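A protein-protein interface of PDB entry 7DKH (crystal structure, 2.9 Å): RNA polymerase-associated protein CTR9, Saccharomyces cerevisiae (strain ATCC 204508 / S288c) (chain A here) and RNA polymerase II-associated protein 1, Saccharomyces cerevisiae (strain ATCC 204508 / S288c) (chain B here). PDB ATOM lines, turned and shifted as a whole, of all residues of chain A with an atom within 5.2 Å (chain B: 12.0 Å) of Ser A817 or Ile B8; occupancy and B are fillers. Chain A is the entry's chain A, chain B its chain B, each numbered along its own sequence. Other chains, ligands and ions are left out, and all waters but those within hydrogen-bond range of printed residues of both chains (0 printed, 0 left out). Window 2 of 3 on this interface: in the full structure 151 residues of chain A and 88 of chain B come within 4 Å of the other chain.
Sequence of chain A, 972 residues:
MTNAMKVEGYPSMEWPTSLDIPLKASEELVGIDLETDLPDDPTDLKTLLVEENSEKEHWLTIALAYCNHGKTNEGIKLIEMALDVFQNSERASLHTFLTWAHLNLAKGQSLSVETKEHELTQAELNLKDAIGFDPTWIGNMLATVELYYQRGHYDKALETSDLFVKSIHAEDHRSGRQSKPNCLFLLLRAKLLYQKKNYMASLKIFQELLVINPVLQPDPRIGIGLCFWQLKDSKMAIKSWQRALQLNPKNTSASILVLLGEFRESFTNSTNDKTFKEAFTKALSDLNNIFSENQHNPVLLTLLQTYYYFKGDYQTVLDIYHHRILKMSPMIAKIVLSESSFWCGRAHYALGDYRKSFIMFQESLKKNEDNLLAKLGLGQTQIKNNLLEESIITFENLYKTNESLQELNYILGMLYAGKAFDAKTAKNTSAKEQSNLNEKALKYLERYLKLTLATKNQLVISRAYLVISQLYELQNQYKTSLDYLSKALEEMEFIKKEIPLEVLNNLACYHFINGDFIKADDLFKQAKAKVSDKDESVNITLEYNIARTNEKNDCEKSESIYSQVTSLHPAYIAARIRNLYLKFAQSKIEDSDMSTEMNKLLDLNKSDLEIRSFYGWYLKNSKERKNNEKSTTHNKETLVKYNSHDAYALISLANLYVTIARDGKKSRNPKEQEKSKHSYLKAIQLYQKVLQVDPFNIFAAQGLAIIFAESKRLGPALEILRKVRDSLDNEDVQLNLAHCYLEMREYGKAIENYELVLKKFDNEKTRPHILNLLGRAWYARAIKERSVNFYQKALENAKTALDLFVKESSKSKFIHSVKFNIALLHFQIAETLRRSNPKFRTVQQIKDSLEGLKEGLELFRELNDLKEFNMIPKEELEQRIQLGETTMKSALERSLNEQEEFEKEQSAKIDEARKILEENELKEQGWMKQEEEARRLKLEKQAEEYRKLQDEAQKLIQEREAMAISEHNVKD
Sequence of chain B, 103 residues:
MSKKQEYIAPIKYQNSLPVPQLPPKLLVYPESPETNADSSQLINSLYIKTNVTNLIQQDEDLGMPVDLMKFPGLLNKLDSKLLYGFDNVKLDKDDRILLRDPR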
ATOM      1  N   ASN A 772       0.115 -16.004  27.506  1.00  0.00           N
ATOM      2  CA  ASN A 772      -1.220 -15.427  27.353  1.00  0.00           C
ATOM      3  C   ASN A 772      -2.022 -16.146  26.271  1.00  0.00           C
ATOM      4  O   ASN A 772      -3.245 -16.293  26.390  1.00  0.00           O
ATOM      5  CB  ASN A 772      -1.105 -13.934  27.037  1.00  0.00           C
ATOM      6  CG  ASN A 772      -2.403 -13.183  27.265  1.00  0.00           C
ATOM      7  OD1 ASN A 772      -3.052 -13.342  28.299  1.00  0.00           O
ATOM      8  ND2 ASN A 772      -2.787 -12.358  26.299  1.00  0.00           N
ATOM      9  N   SER A 812       1.802  -1.156  29.232  1.00  0.00           N
ATOM     10  CA  SER A 812       0.609  -1.243  30.062  1.00  0.00           C
ATOM     11  C   SER A 812      -0.598  -1.733  29.275  1.00  0.00           C
ATOM     12  O   SER A 812      -1.575  -2.184  29.880  1.00  0.00           O
ATOM     13  CB  SER A 812       0.316   0.121  30.690  1.00  0.00           C
ATOM     14  OG  SER A 812      -0.606   0.853  29.904  1.00  0.00           O
ATOM     15  N   LYS A 813      -0.553  -1.637  27.944  1.00  0.00           N
ATOM     16  CA  LYS A 813      -1.496  -2.356  27.092  1.00  0.00           C
ATOM     17  C   LYS A 813      -1.573  -3.827  27.494  1.00  0.00           C
ATOM     18  O   LYS A 813      -2.649  -4.347  27.825  1.00  0.00           O
ATOM     19  CB  LYS A 813      -1.078  -2.179  25.626  1.00  0.00           C
ATOM     20  CG  LYS A 813      -1.589  -3.216  24.649  1.00  0.00           C
ATOM     21  CD  LYS A 813      -1.502  -2.694  23.210  1.00  0.00           C
ATOM     22  CE  LYS A 813      -0.069  -2.385  22.794  1.00  0.00           C
ATOM     23  NZ  LYS A 813      -0.012  -1.813  21.417  1.00  0.00           N
ATOM     24  N   PHE A 814      -0.416  -4.496  27.533  1.00  0.00           N
ATOM     25  CA  PHE A 814      -0.384  -5.933  27.784  1.00  0.00           C
ATOM     26  C   PHE A 814      -0.742  -6.249  29.231  1.00  0.00           C
ATOM     27  O   PHE A 814      -1.423  -7.245  29.507  1.00  0.00           O
ATOM     28  CB  PHE A 814       1.002  -6.490  27.445  1.00  0.00           C
ATOM     29  CG  PHE A 814       1.447  -6.213  26.034  1.00  0.00           C
ATOM     30  CD1 PHE A 814       0.587  -6.410  24.964  1.00  0.00           C
ATOM     31  CD2 PHE A 814       2.734  -5.763  25.779  1.00  0.00           C
ATOM     32  CE1 PHE A 814       1.002  -6.156  23.668  1.00  0.00           C
ATOM     33  CE2 PHE A 814       3.152  -5.508  24.484  1.00  0.00           C
ATOM     34  CZ  PHE A 814       2.286  -5.705  23.430  1.00  0.00           C
ATOM     35  N   ILE A 815      -0.300  -5.409  30.173  1.00  0.00           N
ATOM     36  CA  ILE A 815      -0.600  -5.666  31.580  1.00  0.00           C
ATOM     37  C   ILE A 815      -2.091  -5.511  31.838  1.00  0.00           C
ATOM     38  O   ILE A 815      -2.702  -6.330  32.539  1.00  0.00           O
ATOM     39  CB  ILE A 815       0.231  -4.742  32.490  1.00  0.00           C
ATOM     40  CG1 ILE A 815       1.705  -5.143  32.455  1.00  0.00           C
ATOM     41  CG2 ILE A 815      -0.306  -4.770  33.914  1.00  0.00           C
ATOM     42  CD1 ILE A 815       2.632  -4.082  33.005  1.00  0.00           C
ATOM     43  N   HIS A 816      -2.711  -4.478  31.258  1.00  0.00           N
ATOM     44  CA  HIS A 816      -4.152  -4.322  31.406  1.00  0.00           C
ATOM     45  C   HIS A 816      -4.885  -5.483  30.748  1.00  0.00           C
ATOM     46  O   HIS A 816      -5.889  -5.976  31.278  1.00  0.00           O
ATOM     47  CB  HIS A 816      -4.621  -2.992  30.814  1.00  0.00           C
ATOM     48  CG  HIS A 816      -3.985  -1.786  31.436  1.00  0.00           C
ATOM     49  ND1 HIS A 816      -3.909  -0.572  30.788  1.00  0.00           N
ATOM     50  CD2 HIS A 816      -3.384  -1.611  32.636  1.00  0.00           C
ATOM     51  CE1 HIS A 816      -3.296   0.303  31.567  1.00  0.00           C
ATOM     52  NE2 HIS A 816      -2.966  -0.302  32.693  1.00  0.00           N
ATOM     53  N   SER A 817      -4.369  -5.966  29.612  1.00  0.00           N
ATOM     54  CA  SER A 817      -5.051  -7.059  28.930  1.00  0.00           C
ATOM     55  C   SER A 817      -5.002  -8.338  29.755  1.00  0.00           C
ATOM     56  O   SER A 817      -6.003  -9.058  29.860  1.00  0.00           O
ATOM     57  CB  SER A 817      -4.426  -7.288  27.551  1.00  0.00           C
ATOM     58  OG  SER A 817      -4.047  -6.063  26.945  1.00  0.00           O
ATOM     59  N   VAL A 818      -3.869  -8.613  30.399  1.00  0.00           N
ATOM     60  CA  VAL A 818      -3.796  -9.840  31.184  1.00  0.00           C
ATOM     61  C   VAL A 818      -4.519  -9.689  32.527  1.00  0.00           C
ATOM     62  O   VAL A 818      -5.055 -10.672  33.055  1.00  0.00           O
ATOM     63  CB  VAL A 818      -2.336 -10.293  31.355  1.00  0.00           C
ATOM     64  CG1 VAL A 818      -2.299 -11.679  31.936  1.00  0.00           C
ATOM     65  CG2 VAL A 818      -1.635 -10.307  30.005  1.00  0.00           C
ATOM     66  N   LYS A 819      -4.582  -8.476  33.086  1.00  0.00           N
ATOM     67  CA  LYS A 819      -5.406  -8.256  34.274  1.00  0.00           C
ATOM     68  C   LYS A 819      -6.876  -8.523  33.970  1.00  0.00           C
ATOM     69  O   LYS A 819      -7.576  -9.201  34.740  1.00  0.00           O
ATOM     70  CB  LYS A 819      -5.219  -6.829  34.794  1.00  0.00           C
ATOM     71  CG  LYS A 819      -3.900  -6.600  35.488  1.00  0.00           C
ATOM     72  CD  LYS A 819      -3.681  -5.150  35.881  1.00  0.00           C
ATOM     73  CE  LYS A 819      -2.719  -5.052  37.060  1.00  0.00           C
ATOM     74  NZ  LYS A 819      -2.427  -3.646  37.456  1.00  0.00           N
ATOM     75  N   PHE A 820      -7.355  -8.003  32.834  1.00  0.00           N
ATOM     76  CA  PHE A 820      -8.707  -8.316  32.383  1.00  0.00           C
ATOM     77  C   PHE A 820      -8.893  -9.814  32.190  1.00  0.00           C
ATOM     78  O   PHE A 820      -9.944 -10.362  32.538  1.00  0.00           O
ATOM     79  CB  PHE A 820      -9.017  -7.575  31.083  1.00  0.00           C
ATOM     80  CG  PHE A 820     -10.367  -7.900  30.510  1.00  0.00           C
ATOM     81  CD1 PHE A 820     -11.488  -7.191  30.912  1.00  0.00           C
ATOM     82  CD2 PHE A 820     -10.520  -8.923  29.584  1.00  0.00           C
ATOM     83  CE1 PHE A 820     -12.733  -7.487  30.397  1.00  0.00           C
ATOM     84  CE2 PHE A 820     -11.767  -9.227  29.065  1.00  0.00           C
ATOM     85  CZ  PHE A 820     -12.873  -8.507  29.471  1.00  0.00           C
ATOM     86  N   ASN A 821      -7.896 -10.490  31.610  1.00  0.00           N
ATOM     87  CA  ASN A 821      -8.017 -11.929  31.395  1.00  0.00           C
ATOM     88  C   ASN A 821      -8.185 -12.672  32.713  1.00  0.00           C
ATOM     89  O   ASN A 821      -9.044 -13.552  32.842  1.00  0.00           O
ATOM     90  CB  ASN A 821      -6.793 -12.445  30.650  1.00  0.00           C
ATOM     91  CG  ASN A 821      -6.820 -12.082  29.193  1.00  0.00           C
ATOM     92  OD1 ASN A 821      -7.880 -12.047  28.576  1.00  0.00           O
ATOM     93  ND2 ASN A 821      -5.654 -11.782  28.634  1.00  0.00           N
ATOM     94  N   MET A 871     -10.761  -1.417  26.021  1.00  0.00           N
ATOM     95  CA  MET A 871     -10.926  -2.680  25.312  1.00  0.00           C
ATOM     96  C   MET A 871     -12.302  -3.290  25.555  1.00  0.00           C
ATOM     97  O   MET A 871     -12.821  -4.001  24.687  1.00  0.00           O
ATOM     98  CB  MET A 871      -9.849  -3.664  25.762  1.00  0.00           C
ATOM     99  CG  MET A 871      -8.440  -3.253  25.363  1.00  0.00           C
ATOM    100  SD  MET A 871      -8.178  -3.054  23.474  1.00  0.00           S
ATOM    101  CE  MET A 871      -8.344  -4.930  22.971  1.00  0.00           C
ATOM    102  N   GLN B   5     -14.481 -16.115  23.871  1.00  0.00           N
ATOM    103  CA  GLN B   5     -15.329 -15.162  23.166  1.00  0.00           C
ATOM    104  C   GLN B   5     -14.861 -13.744  23.453  1.00  0.00           C
ATOM    105  O   GLN B   5     -14.980 -12.837  22.625  1.00  0.00           O
ATOM    106  CB  GLN B   5     -16.783 -15.305  23.609  1.00  0.00           C
ATOM    107  CG  GLN B   5     -17.482 -16.581  23.190  1.00  0.00           C
ATOM    108  CD  GLN B   5     -18.841 -16.706  23.850  1.00  0.00           C
ATOM    109  OE1 GLN B   5     -19.480 -15.700  24.164  1.00  0.00           O
ATOM    110  NE2 GLN B   5     -19.273 -17.937  24.102  1.00  0.00           N
ATOM    111  N   GLU B   6     -14.318 -13.579  24.656  1.00  0.00           N
ATOM    112  CA  GLU B   6     -13.960 -12.274  25.179  1.00  0.00           C
ATOM    113  C   GLU B   6     -12.555 -12.241  25.748  1.00  0.00           C
ATOM    114  O   GLU B   6     -12.136 -11.198  26.259  1.00  0.00           O
ATOM    115  CB  GLU B   6     -14.956 -11.825  26.257  1.00  0.00           C
ATOM    116  CG  GLU B   6     -15.340 -10.362  26.130  1.00  0.00           C
ATOM    117  CD  GLU B   6     -16.290  -9.909  27.217  1.00  0.00           C
ATOM    118  OE1 GLU B   6     -16.593  -8.697  27.280  1.00  0.00           O
ATOM    119  OE2 GLU B   6     -16.737 -10.765  28.009  1.00  0.00           O
ATOM    120  N   TYR B   7     -11.825 -13.348  25.694  1.00  0.00           N
ATOM    121  CA  TYR B   7     -10.452 -13.357  26.171  1.00  0.00           C
ATOM    122  C   TYR B   7      -9.573 -12.609  25.181  1.00  0.00           C
ATOM    123  O   TYR B   7      -9.614 -12.865  23.973  1.00  0.00           O
ATOM    124  CB  TYR B   7      -9.965 -14.795  26.346  1.00  0.00           C
ATOM    125  CG  TYR B   7      -8.658 -14.955  27.101  1.00  0.00           C
ATOM    126  CD1 TYR B   7      -7.439 -14.678  26.487  1.00  0.00           C
ATOM    127  CD2 TYR B   7      -8.639 -15.420  28.413  1.00  0.00           C
ATOM    128  CE1 TYR B   7      -6.241 -14.839  27.160  1.00  0.00           C
ATOM    129  CE2 TYR B   7      -7.442 -15.587  29.098  1.00  0.00           C
ATOM    130  CZ  TYR B   7      -6.246 -15.294  28.462  1.00  0.00           C
ATOM    131  OH  TYR B   7      -5.043 -15.449  29.116  1.00  0.00           O
ATOM    132  N   ILE B   8      -8.772 -11.691  25.704  1.00  0.00           N
ATOM    133  CA  ILE B   8      -8.036 -10.725  24.900  1.00  0.00           C
ATOM    134  C   ILE B   8      -6.587 -11.191  24.813  1.00  0.00           C
ATOM    135  O   ILE B   8      -5.847 -11.165  25.803  1.00  0.00           O
ATOM    136  CB  ILE B   8      -8.155  -9.313  25.488  1.00  0.00           C
ATOM    137  CG1 ILE B   8      -7.118  -8.374  24.874  1.00  0.00           C
ATOM    138  CG2 ILE B   8      -8.054  -9.352  27.008  1.00  0.00           C
ATOM    139  CD1 ILE B   8      -7.250  -6.963  25.359  1.00  0.00           C
ATOM    140  N   ALA B   9      -6.193 -11.633  23.621  1.00  0.00           N
ATOM    141  CA  ALA B   9      -4.879 -12.186  23.324  1.00  0.00           C
ATOM    142  C   ALA B   9      -4.654 -12.119  21.819  1.00  0.00           C
ATOM    143  O   ALA B   9      -4.979 -13.074  21.103  1.00  0.00           O
ATOM    144  CB  ALA B   9      -4.756 -13.627  23.815  1.00  0.00           C
ATOM    145  N   PRO B  10      -4.122 -11.018  21.298  1.00  0.00           N
ATOM    146  CA  PRO B  10      -4.013 -10.881  19.842  1.00  0.00           C
ATOM    147  C   PRO B  10      -3.005 -11.855  19.256  1.00  0.00           C
ATOM    148  O   PRO B  10      -1.977 -12.170  19.862  1.00  0.00           O
ATOM    149  CB  PRO B  10      -3.549  -9.434  19.663  1.00  0.00           C
ATOM    150  CG  PRO B  10      -2.786  -9.148  20.914  1.00  0.00           C
ATOM    151  CD  PRO B  10      -3.481  -9.902  22.011  1.00  0.00           C
ATOM    152  N   ILE B  11      -3.308 -12.318  18.049  1.00  0.00           N
ATOM    153  CA  ILE B  11      -2.445 -13.237  17.319  1.00  0.00           C
ATOM    154  C   ILE B  11      -1.647 -12.439  16.297  1.00  0.00           C
ATOM    155  O   ILE B  11      -2.217 -11.637  15.547  1.00  0.00           O
ATOM    156  CB  ILE B  11      -3.271 -14.344  16.641  1.00  0.00           C
ATOM    157  CG1 ILE B  11      -3.996 -15.177  17.698  1.00  0.00           C
ATOM    158  CG2 ILE B  11      -2.393 -15.214  15.773  1.00  0.00           C
ATOM    159  CD1 ILE B  11      -4.846 -16.294  17.137  1.00  0.00           C
ATOM    160  N   LYS B  12      -0.330 -12.652  16.265  1.00  0.00           N
ATOM    161  CA  LYS B  12       0.540 -11.936  15.335  1.00  0.00           C
ATOM    162  C   LYS B  12       1.487 -12.945  14.697  1.00  0.00           C
ATOM    163  O   LYS B  12       2.425 -13.421  15.343  1.00  0.00           O
ATOM    164  CB  LYS B  12       1.317 -10.811  16.019  1.00  0.00           C
ATOM    165  CG  LYS B  12       1.673 -11.016  17.498  1.00  0.00           C
ATOM    166  CD  LYS B  12       2.119  -9.684  18.117  1.00  0.00           C
ATOM    167  CE  LYS B  12       2.249  -9.711  19.639  1.00  0.00           C
ATOM    168  NZ  LYS B  12       3.377 -10.587  20.060  1.00  0.00           N
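The side-chain hydroxyl (OH) of Tyr B7 is in hydrogen-bond range of the side-chain amide oxygen (OD1) of Asn A772, at 3.0 Å.
ND2 of Asn A772 lies within hydrogen-bond range of O of Ile B8 (3.3 Å).
The backbone carbonyl oxygen of Ile B8 lies within hydrogen-bond range of the side-chain amide nitrogen of Asn A821 (2.9 Å).
Among the printed residues, pairs that only touch across the chains: Met A871 with Ile B8 (3.3 Å), Asn A821 with Tyr B7 (3.3 Å), Asn A772 with Ala B9 (3.4 Å), Phe A820 with Glu B6 (3.4 Å), Ser A817 with Ile B8 (3.5 Å) and Phe A820 with Ile B8 (3.6 Å).
ND2 of Asn A821 is in hydrogen-bond range of OD1 of Asn A772, 3.1 Å away.
The side-chain amide nitrogen (ND2) of Asn A821 lies within hydrogen-bond range of the backbone carbonyl oxygen (O) of Ser A817 (3.0 Å).
No residue of chain B comes within 4 Å of His A816.
Ser A817 touches one residue of chain B.
No residue of chain B comes within 4 Å of Val A818.
Phe A820 touches two residues of chain B.
Of chain B, only Ile B8 (3.3 Å) comes within 4 Å of Met A871.
Of the printed residues of chain A, Glu B6 touches Phe A820 (3.4 Å).
Printed residues of chain A within 4 Å of Tyr B7: Asn A772 and Asn A821.
Of chain A, only Asn A772 (3.3 Å), Ser A817 (3.5 Å), Phe A820 (3.6 Å), Asn A821 (2.9 Å) and Met A871 (3.3 Å) come within 4 Å of Ile B8.
Of the printed residues of chain A, Ala B9 touches Asn A772 (3.4 Å).
The nearest residue of chain B that does not touch Ser A817 is Ala B9 (6.1 Å).
The nearest printed residue of chain A that does not touch Ala B9 is Asn A821 (5.0 Å).
Hydrophobic or aromatic side chains of chain B within 4 Å of the printed part of chain A: Tyr B7, Ile B8 and Ala B9.
Of the 12 printed residues of chain A, 5 touch a printed residue of chain B.
Hydrophobic or aromatic side chains of chain A within 4 Å of the printed part of chain B: Phe A820 and Met A871.
Along chain A the printed residues that touch a printed residue of chain B span positions 772 to 871.
Among the printed residues, 9 pairs touch across the chains.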
